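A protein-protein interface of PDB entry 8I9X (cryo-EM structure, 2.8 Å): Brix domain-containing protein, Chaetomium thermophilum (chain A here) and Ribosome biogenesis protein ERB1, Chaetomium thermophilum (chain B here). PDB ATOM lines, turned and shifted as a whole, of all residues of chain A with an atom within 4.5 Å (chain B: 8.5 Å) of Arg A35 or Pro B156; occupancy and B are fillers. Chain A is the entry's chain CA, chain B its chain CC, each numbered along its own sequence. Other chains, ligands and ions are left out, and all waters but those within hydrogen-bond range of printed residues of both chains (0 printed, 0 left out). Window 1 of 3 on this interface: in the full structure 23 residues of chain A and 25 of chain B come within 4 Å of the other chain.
Printed residues of chain A that touch a printed residue of chain B: Lys A33, Arg A35, Arg A63, Asn A85, Cys A86 and Asn A87. Hydrophobic or aromatic side chains of chain B within 4 Å of the printed part of chain A: Ile B154, Pro B156, Val B157 and Tyr B158. Among the printed residues, 16 pairs touch across the chains.
The side-chain amino group (NZ) of Lys A33 is in salt-bridge range of the side-chain carboxylate (OD1) of Asp B155 (3.3 Å). The backbone carbonyl oxygen (O) of Val B157 sits at hydrogen-bond distance from the guanidinium group (NH1) of Arg A35, at 3.0 Å. The guanidinium group of Arg A35 is in salt-bridge range of the side-chain carboxylate of Asp B162 (3.5 Å). NE of Arg A63 lies within salt-bridge range of OD1 of Asp B162 (3.7 Å). NH1 of Arg A63 sits close to O3P of TPO B163. The side-chain amide nitrogen (ND2) of Asn A85 sits close to the backbone carbonyl oxygen (O) of Val B157, at 3.5 Å. The side-chain amide nitrogen (ND2) of Asn A85 sits at hydrogen-bond distance from the side-chain carboxylate (OD1) of Asp B159 (3.0 Å).
Lys A33 touches Pro B156. Val B157 touches Lys A33 (CG1 to NZ, 3.6 Å). N of Arg A35 touches CB of Pro B156, at 3.97 Å. NH1 of Arg A35 touches CD2 of Tyr B158 (3.6 Å). CA of Asn A85 touches CG2 of Ile B154, at 3.9 Å. Asn A85 touches Asp B155. O of Asn A85 touches CA of Pro B156, at 3.6 Å. Cys A86 touches Ile B154. CG of Pro B156 touches CG of Asn A87, 3.6 Å away.
The backbone NH of Arg A35 lies within hydrogen-bond range of the side-chain amide oxygen of Asn A87, at 2.8 Å. The backbone carbonyl oxygen of Arg A35 sits at hydrogen-bond distance from the side-chain amide nitrogen of Asn A88 (2.9 Å). The backbone carbonyl oxygen (O) of Val A36 lies within hydrogen-bond range of the backbone NH (N) of Arg A63, 3.1 Å away. SG of Cys A86 sits at hydrogen-bond distance from O of Tyr A84, at 3.6 Å. ND2 of Asn A88 is in hydrogen-bond range of OD1 of Asn A87 (2.9 Å). The backbone NH (N) of Asp B164 sits close to the side-chain carboxylate (OD2) of Asp B162 (3.1 Å).
Arg A35 touches just these residues of chain B: Pro B156 (3.97 Å), Val B157 (3.0 Å), Tyr B158 (3.6 Å) and Asp B162 (3.5 Å). Pro B156 touches just these residues of chain A: Lys A33, Arg A35, Asn A85 and Asn A87. Printed residues of chain A within 4 Å of TPO B163: Arg A63 (2.7 Å). Of the printed residues of chain A, Tyr B158 touches Arg A35. Printed residues of chain A within 4 Å of Asp B155: Lys A33 and Asn A85. Of the printed residues of chain B, Asn A87 touches Pro B156 (3.6 Å). Asn A88 touches none of the printed residues of chain B. His A61 touches none of the printed residues of chain B. The nearest residue of chain A that does not touch Pro B156 is Gln A34 (4.1 Å).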
ATOM      1  N   LYS A  33     -10.000   4.885  -3.178  1.00  0.00           N
ATOM      2  CA  LYS A  33      -8.718   4.223  -2.846  1.00  0.00           C
ATOM      3  C   LYS A  33      -8.017   3.888  -4.158  1.00  0.00           C
ATOM      4  O   LYS A  33      -8.412   2.897  -4.782  1.00  0.00           O
ATOM      5  CB  LYS A  33      -9.001   3.028  -1.929  1.00  0.00           C
ATOM      6  CG  LYS A  33      -9.987   3.279  -0.802  1.00  0.00           C
ATOM      7  CD  LYS A  33     -10.437   2.002  -0.142  1.00  0.00           C
ATOM      8  CE  LYS A  33      -9.388   1.434   0.785  1.00  0.00           C
ATOM      9  NZ  LYS A  33      -9.963   0.417   1.695  1.00  0.00           N
ATOM     10  N   GLN A  34      -7.110   4.747  -4.611  1.00  0.00           N
ATOM     11  CA  GLN A  34      -6.356   4.496  -5.857  1.00  0.00           C
ATOM     12  C   GLN A  34      -4.868   4.583  -5.557  1.00  0.00           C
ATOM     13  O   GLN A  34      -4.475   5.556  -4.910  1.00  0.00           O
ATOM     14  CB  GLN A  34      -6.709   5.495  -6.956  1.00  0.00           C
ATOM     15  CG  GLN A  34      -8.196   5.685  -7.182  1.00  0.00           C
ATOM     16  CD  GLN A  34      -8.727   4.884  -8.342  1.00  0.00           C
ATOM     17  OE1 GLN A  34      -8.061   4.005  -8.877  1.00  0.00           O
ATOM     18  NE2 GLN A  34      -9.950   5.187  -8.742  1.00  0.00           N
ATOM     19  N   ARG A  35      -4.076   3.620  -6.020  1.00  0.00           N
ATOM     20  CA  ARG A  35      -2.591   3.642  -5.845  1.00  0.00           C
ATOM     21  C   ARG A  35      -1.881   3.328  -7.164  1.00  0.00           C
ATOM     22  O   ARG A  35      -2.343   2.422  -7.863  1.00  0.00           O
ATOM     23  CB  ARG A  35      -2.166   2.624  -4.792  1.00  0.00           C
ATOM     24  CG  ARG A  35      -2.171   3.129  -3.359  1.00  0.00           C
ATOM     25  CD  ARG A  35      -1.663   2.055  -2.423  1.00  0.00           C
ATOM     26  NE  ARG A  35      -0.220   1.919  -2.496  1.00  0.00           N
ATOM     27  CZ  ARG A  35       0.501   1.134  -1.714  1.00  0.00           C
ATOM     28  NH1 ARG A  35      -0.088   0.389  -0.797  1.00  0.00           N
ATOM     29  NH2 ARG A  35       1.810   1.081  -1.861  1.00  0.00           N
ATOM     30  N   VAL A  36      -0.772   4.007  -7.470  1.00  0.00           N
ATOM     31  CA  VAL A  36      -0.114   3.813  -8.802  1.00  0.00           C
ATOM     32  C   VAL A  36       1.290   3.220  -8.668  1.00  0.00           C
ATOM     33  O   VAL A  36       1.958   3.510  -7.697  1.00  0.00           O
ATOM     34  CB  VAL A  36      -0.104   5.096  -9.657  1.00  0.00           C
ATOM     35  CG1 VAL A  36       0.236   4.825 -11.114  1.00  0.00           C
ATOM     36  CG2 VAL A  36      -1.398   5.875  -9.560  1.00  0.00           C
ATOM     37  N   LEU A  37       1.675   2.317  -9.561  1.00  0.00           N
ATOM     38  CA  LEU A  37       3.066   1.818  -9.580  1.00  0.00           C
ATOM     39  C   LEU A  37       3.718   2.430 -10.815  1.00  0.00           C
ATOM     40  O   LEU A  37       3.367   2.017 -11.918  1.00  0.00           O
ATOM     41  CB  LEU A  37       3.068   0.294  -9.673  1.00  0.00           C
ATOM     42  CG  LEU A  37       4.445  -0.363  -9.608  1.00  0.00           C
ATOM     43  CD1 LEU A  37       5.076  -0.170  -8.239  1.00  0.00           C
ATOM     44  CD2 LEU A  37       4.358  -1.838  -9.953  1.00  0.00           C
ATOM     45  N   HIS A  61       0.208   9.212  -4.404  1.00  0.00           N
ATOM     46  CA  HIS A  61      -0.345   7.853  -4.187  1.00  0.00           C
ATOM     47  C   HIS A  61       0.429   6.811  -4.985  1.00  0.00           C
ATOM     48  O   HIS A  61       0.032   5.646  -4.933  1.00  0.00           O
ATOM     49  CB  HIS A  61      -1.824   7.840  -4.556  1.00  0.00           C
ATOM     50  CG  HIS A  61      -2.164   8.319  -5.922  1.00  0.00           C
ATOM     51  ND1 HIS A  61      -1.910   9.599  -6.351  1.00  0.00           N
ATOM     52  CD2 HIS A  61      -2.797   7.700  -6.937  1.00  0.00           C
ATOM     53  CE1 HIS A  61      -2.332   9.738  -7.585  1.00  0.00           C
ATOM     54  NE2 HIS A  61      -2.886   8.591  -7.963  1.00  0.00           N
ATOM     55  N   ARG A  63       4.271   5.029  -6.327  1.00  0.00           N
ATOM     56  CA  ARG A  63       5.649   4.797  -5.929  1.00  0.00           C
ATOM     57  C   ARG A  63       6.461   4.277  -7.112  1.00  0.00           C
ATOM     58  O   ARG A  63       5.903   3.665  -8.034  1.00  0.00           O
ATOM     59  CB  ARG A  63       5.723   3.819  -4.757  1.00  0.00           C
ATOM     60  CG  ARG A  63       5.421   2.378  -5.022  1.00  0.00           C
ATOM     61  CD  ARG A  63       5.050   1.716  -3.693  1.00  0.00           C
ATOM     62  NE  ARG A  63       6.129   1.574  -2.747  1.00  0.00           N
ATOM     63  CZ  ARG A  63       7.265   0.911  -2.940  1.00  0.00           C
ATOM     64  NH1 ARG A  63       8.239   0.906  -2.039  1.00  0.00           N
ATOM     65  NH2 ARG A  63       7.436   0.197  -4.043  1.00  0.00           N
ATOM     66  N   TYR A  84       2.595  -4.564  -4.331  1.00  0.00           N
ATOM     67  CA  TYR A  84       2.629  -3.219  -3.702  1.00  0.00           C
ATOM     68  C   TYR A  84       1.211  -2.681  -3.551  1.00  0.00           C
ATOM     69  O   TYR A  84       1.088  -1.501  -3.226  1.00  0.00           O
ATOM     70  CB  TYR A  84       3.523  -2.293  -4.520  1.00  0.00           C
ATOM     71  CG  TYR A  84       4.981  -2.654  -4.522  1.00  0.00           C
ATOM     72  CD1 TYR A  84       5.618  -3.041  -5.687  1.00  0.00           C
ATOM     73  CD2 TYR A  84       5.724  -2.610  -3.359  1.00  0.00           C
ATOM     74  CE1 TYR A  84       6.960  -3.370  -5.698  1.00  0.00           C
ATOM     75  CE2 TYR A  84       7.068  -2.937  -3.353  1.00  0.00           C
ATOM     76  CZ  TYR A  84       7.688  -3.317  -4.526  1.00  0.00           C
ATOM     77  OH  TYR A  84       9.013  -3.641  -4.524  1.00  0.00           O
ATOM     78  N   ASN A  85       0.198  -3.499  -3.798  1.00  0.00           N
ATOM     79  CA  ASN A  85      -1.234  -3.124  -3.630  1.00  0.00           C
ATOM     80  C   ASN A  85      -1.538  -1.922  -4.515  1.00  0.00           C
ATOM     81  O   ASN A  85      -2.180  -0.991  -4.025  1.00  0.00           O
ATOM     82  CB  ASN A  85      -1.616  -2.995  -2.153  1.00  0.00           C
ATOM     83  CG  ASN A  85      -1.187  -4.173  -1.312  1.00  0.00           C
ATOM     84  OD1 ASN A  85      -1.727  -5.264  -1.447  1.00  0.00           O
ATOM     85  ND2 ASN A  85      -0.218  -3.961  -0.440  1.00  0.00           N
ATOM     86  N   CYS A  86      -1.122  -1.981  -5.775  1.00  0.00           N
ATOM     87  CA  CYS A  86      -1.300  -0.852  -6.713  1.00  0.00           C
ATOM     88  C   CYS A  86      -2.329  -1.265  -7.773  1.00  0.00           C
ATOM     89  O   CYS A  86      -2.143  -2.309  -8.387  1.00  0.00           O
ATOM     90  CB  CYS A  86       0.049  -0.436  -7.283  1.00  0.00           C
ATOM     91  SG  CYS A  86       1.012   0.571  -6.127  1.00  0.00           S
ATOM     92  N   ASN A  87      -3.396  -0.497  -7.916  1.00  0.00           N
ATOM     93  CA  ASN A  87      -4.479  -0.811  -8.881  1.00  0.00           C
ATOM     94  C   ASN A  87      -4.241  -0.144 -10.237  1.00  0.00           C
ATOM     95  O   ASN A  87      -4.923  -0.508 -11.168  1.00  0.00           O
ATOM     96  CB  ASN A  87      -5.843  -0.494  -8.268  1.00  0.00           C
ATOM     97  CG  ASN A  87      -6.099   0.964  -7.971  1.00  0.00           C
ATOM     98  OD1 ASN A  87      -5.181   1.720  -7.686  1.00  0.00           O
ATOM     99  ND2 ASN A  87      -7.360   1.354  -8.008  1.00  0.00           N
ATOM    100  N   ASN A  88      -3.305   0.797 -10.326  1.00  0.00           N
ATOM    101  CA  ASN A  88      -3.008   1.503 -11.593  1.00  0.00           C
ATOM    102  C   ASN A  88      -1.511   1.329 -11.877  1.00  0.00           C
ATOM    103  O   ASN A  88      -0.740   1.317 -10.917  1.00  0.00           O
ATOM    104  CB  ASN A  88      -3.485   2.959 -11.571  1.00  0.00           C
ATOM    105  CG  ASN A  88      -4.616   3.275 -10.618  1.00  0.00           C
ATOM    106  OD1 ASN A  88      -5.773   3.020 -10.920  1.00  0.00           O
ATOM    107  ND2 ASN A  88      -4.301   3.880  -9.486  1.00  0.00           N
ATOM    108  N   GLU B 153     -10.163  -8.439  -7.476  1.00  0.00           N
ATOM    109  CA  GLU B 153      -9.692  -7.032  -7.479  1.00  0.00           C
ATOM    110  C   GLU B 153      -8.738  -6.738  -6.326  1.00  0.00           C
ATOM    111  O   GLU B 153      -8.720  -7.511  -5.358  1.00  0.00           O
ATOM    112  CB  GLU B 153     -10.892  -6.084  -7.476  1.00  0.00           C
ATOM    113  CG  GLU B 153     -11.782  -6.246  -8.689  1.00  0.00           C
ATOM    114  CD  GLU B 153     -11.675  -5.120  -9.700  1.00  0.00           C
ATOM    115  OE1 GLU B 153     -10.543  -4.780 -10.086  1.00  0.00           O
ATOM    116  OE2 GLU B 153     -12.725  -4.584 -10.094  1.00  0.00           O
ATOM    117  N   ILE B 154      -7.979  -5.647  -6.435  1.00  0.00           N
ATOM    118  CA  ILE B 154      -6.967  -5.266  -5.416  1.00  0.00           C
ATOM    119  C   ILE B 154      -7.556  -4.212  -4.483  1.00  0.00           C
ATOM    120  O   ILE B 154      -8.286  -3.342  -4.990  1.00  0.00           O
ATOM    121  CB  ILE B 154      -5.717  -4.677  -6.111  1.00  0.00           C
ATOM    122  CG1 ILE B 154      -5.313  -5.449  -7.366  1.00  0.00           C
ATOM    123  CG2 ILE B 154      -4.555  -4.545  -5.138  1.00  0.00           C
ATOM    124  CD1 ILE B 154      -3.827  -5.506  -7.587  1.00  0.00           C
ATOM    125  N   ASP B 155      -7.255  -4.262  -3.186  1.00  0.00           N
ATOM    126  CA  ASP B 155      -7.675  -3.186  -2.257  1.00  0.00           C
ATOM    127  C   ASP B 155      -6.497  -2.233  -2.196  1.00  0.00           C
ATOM    128  O   ASP B 155      -5.430  -2.692  -1.764  1.00  0.00           O
ATOM    129  CB  ASP B 155      -7.993  -3.708  -0.856  1.00  0.00           C
ATOM    130  CG  ASP B 155      -8.878  -2.788  -0.037  1.00  0.00           C
ATOM    131  OD1 ASP B 155      -9.442  -1.836  -0.614  1.00  0.00           O
ATOM    132  OD2 ASP B 155      -9.003  -3.034   1.178  1.00  0.00           O
ATOM    133  N   PRO B 156      -6.565  -0.990  -2.697  1.00  0.00           N
ATOM    134  CA  PRO B 156      -5.381  -0.137  -2.648  1.00  0.00           C
ATOM    135  C   PRO B 156      -5.077   0.305  -1.207  1.00  0.00           C
ATOM    136  O   PRO B 156      -5.367   1.429  -0.872  1.00  0.00           O
ATOM    137  CB  PRO B 156      -5.788   0.972  -3.612  1.00  0.00           C
ATOM    138  CG  PRO B 156      -6.824   0.301  -4.470  1.00  0.00           C
ATOM    139  CD  PRO B 156      -7.667  -0.415  -3.444  1.00  0.00           C
ATOM    140  N   VAL B 157      -4.490  -0.583  -0.406  1.00  0.00           N
ATOM    141  CA  VAL B 157      -4.249  -0.300   1.037  1.00  0.00           C
ATOM    142  C   VAL B 157      -2.770  -0.490   1.353  1.00  0.00           C
ATOM    143  O   VAL B 157      -2.097  -1.262   0.666  1.00  0.00           O
ATOM    144  CB  VAL B 157      -5.113  -1.183   1.953  1.00  0.00           C
ATOM    145  CG1 VAL B 157      -6.544  -0.690   2.053  1.00  0.00           C
ATOM    146  CG2 VAL B 157      -5.058  -2.656   1.584  1.00  0.00           C
ATOM    147  N   TYR B 158      -2.300   0.200   2.375  1.00  0.00           N
ATOM    148  CA  TYR B 158      -0.880   0.126   2.760  1.00  0.00           C
ATOM    149  C   TYR B 158      -0.731  -0.955   3.823  1.00  0.00           C
ATOM    150  O   TYR B 158      -1.561  -0.997   4.737  1.00  0.00           O
ATOM    151  CB  TYR B 158      -0.415   1.497   3.244  1.00  0.00           C
ATOM    152  CG  TYR B 158      -0.367   2.555   2.174  1.00  0.00           C
ATOM    153  CD1 TYR B 158      -1.509   3.220   1.763  1.00  0.00           C
ATOM    154  CD2 TYR B 158       0.828   2.883   1.567  1.00  0.00           C
ATOM    155  CE1 TYR B 158      -1.467   4.179   0.769  1.00  0.00           C
ATOM    156  CE2 TYR B 158       0.891   3.844   0.575  1.00  0.00           C
ATOM    157  CZ  TYR B 158      -0.259   4.498   0.179  1.00  0.00           C
ATOM    158  OH  TYR B 158      -0.185   5.440  -0.801  1.00  0.00           O
ATOM    159  N   ASP B 159       0.310  -1.778   3.715  1.00  0.00           N
ATOM    160  CA  ASP B 159       0.579  -2.853   4.697  1.00  0.00           C
ATOM    161  C   ASP B 159       1.638  -2.371   5.700  1.00  0.00           C
ATOM    162  O   ASP B 159       2.212  -1.298   5.458  1.00  0.00           O
ATOM    163  CB  ASP B 159       0.906  -4.122   3.925  1.00  0.00           C
ATOM    164  CG  ASP B 159      -0.282  -4.709   3.187  1.00  0.00           C
ATOM    165  OD1 ASP B 159      -0.051  -5.428   2.199  1.00  0.00           O
ATOM    166  OD2 ASP B 159      -1.427  -4.444   3.602  1.00  0.00           O
ATOM    167  N   ASP B 161       4.629  -2.664   6.262  1.00  0.00           N
ATOM    168  CA  ASP B 161       5.994  -2.923   5.760  1.00  0.00           C
ATOM    169  C   ASP B 161       6.268  -1.831   4.742  1.00  0.00           C
ATOM    170  O   ASP B 161       7.437  -1.652   4.375  1.00  0.00           O
ATOM    171  CB  ASP B 161       6.094  -4.326   5.159  1.00  0.00           C
ATOM    172  CG  ASP B 161       5.167  -4.604   3.988  1.00  0.00           C
ATOM    173  OD1 ASP B 161       4.135  -3.918   3.867  1.00  0.00           O
ATOM    174  OD2 ASP B 161       5.492  -5.510   3.197  1.00  0.00           O
ATOM    175  N   ASP B 162       5.214  -1.137   4.309  1.00  0.00           N
ATOM    176  CA  ASP B 162       5.351  -0.065   3.296  1.00  0.00           C
ATOM    177  C   ASP B 162       5.994   1.170   3.921  1.00  0.00           C
ATOM    178  O   ASP B 162       5.702   1.458   5.079  1.00  0.00           O
ATOM    179  CB  ASP B 162       4.005   0.264   2.645  1.00  0.00           C
ATOM    180  CG  ASP B 162       4.165   0.954   1.304  1.00  0.00           C
ATOM    181  OD1 ASP B 162       4.479   0.254   0.324  1.00  0.00           O
ATOM    182  OD2 ASP B 162       3.995   2.185   1.256  1.00  0.00           O
ATOM    183  N   TPO B 163       6.839   1.861   3.163  1.00  0.00           N
ATOM    184  CA  TPO B 163       7.529   3.091   3.618  1.00  0.00           C
ATOM    185  CB  TPO B 163       8.433   3.565   2.480  1.00  0.00           C
ATOM    186  CG2 TPO B 163       9.334   4.713   2.874  1.00  0.00           C
ATOM    187  OG1 TPO B 163       9.295   2.437   2.131  1.00  0.00           O
ATOM    188  P   TPO B 163       9.118   1.659   0.740  1.00  0.00           P
ATOM    189  O1P TPO B 163       7.801   0.926   0.801  1.00  0.00           O
ATOM    190  O2P TPO B 163      10.293   0.722   0.627  1.00  0.00           O
ATOM    191  O3P TPO B 163       9.133   2.743  -0.307  1.00  0.00           O
ATOM    192  C   TPO B 163       6.500   4.161   3.946  1.00  0.00           C
ATOM    193  O   TPO B 163       6.804   5.031   4.768  1.00  0.00           O
ATOM    194  N   ASP B 164       5.309   4.060   3.358  1.00  0.00           N
ATOM    195  CA  ASP B 164       4.231   5.057   3.552  1.00  0.00           C
ATOM    196  C   ASP B 164       3.084   4.471   4.359  1.00  0.00           C
ATOM    197  O   ASP B 164       1.958   4.872   4.110  1.00  0.00           O
ATOM    198  CB  ASP B 164       3.687   5.545   2.208  1.00  0.00           C
ATOM    199  CG  ASP B 164       4.721   6.229   1.334  1.00  0.00           C
ATOM    200  OD1 ASP B 164       5.709   6.745   1.887  1.00  0.00           O
ATOM    201  OD2 ASP B 164       4.529   6.238   0.107  1.00  0.00           O
ATOM    202  N   TYR B 165       3.353   3.553   5.270  1.00  0.00           N
ATOM    203  CA  TYR B 165       2.270   3.070   6.154  1.00  0.00           C
ATOM    204  C   TYR B 165       1.983   4.157   7.173  1.00  0.00           C
ATOM    205  O   TYR B 165       0.844   4.606   7.267  1.00  0.00           O
ATOM    206  CB  TYR B 165       2.676   1.760   6.826  1.00  0.00           C
ATOM    207  CG  TYR B 165       1.745   1.179   7.856  1.00  0.00           C
ATOM    208  CD1 TYR B 165       0.457   0.800   7.528  1.00  0.00           C
ATOM    209  CD2 TYR B 165       2.183   0.941   9.146  1.00  0.00           C
ATOM    210  CE1 TYR B 165      -0.388   0.245   8.473  1.00  0.00           C
ATOM    211  CE2 TYR B 165       1.354   0.384  10.101  1.00  0.00           C
ATOM    212  CZ  TYR B 165       0.065   0.029   9.760  1.00  0.00           C
ATOM    213  OH  TYR B 165      -0.761  -0.520  10.696  1.00  0.00           O
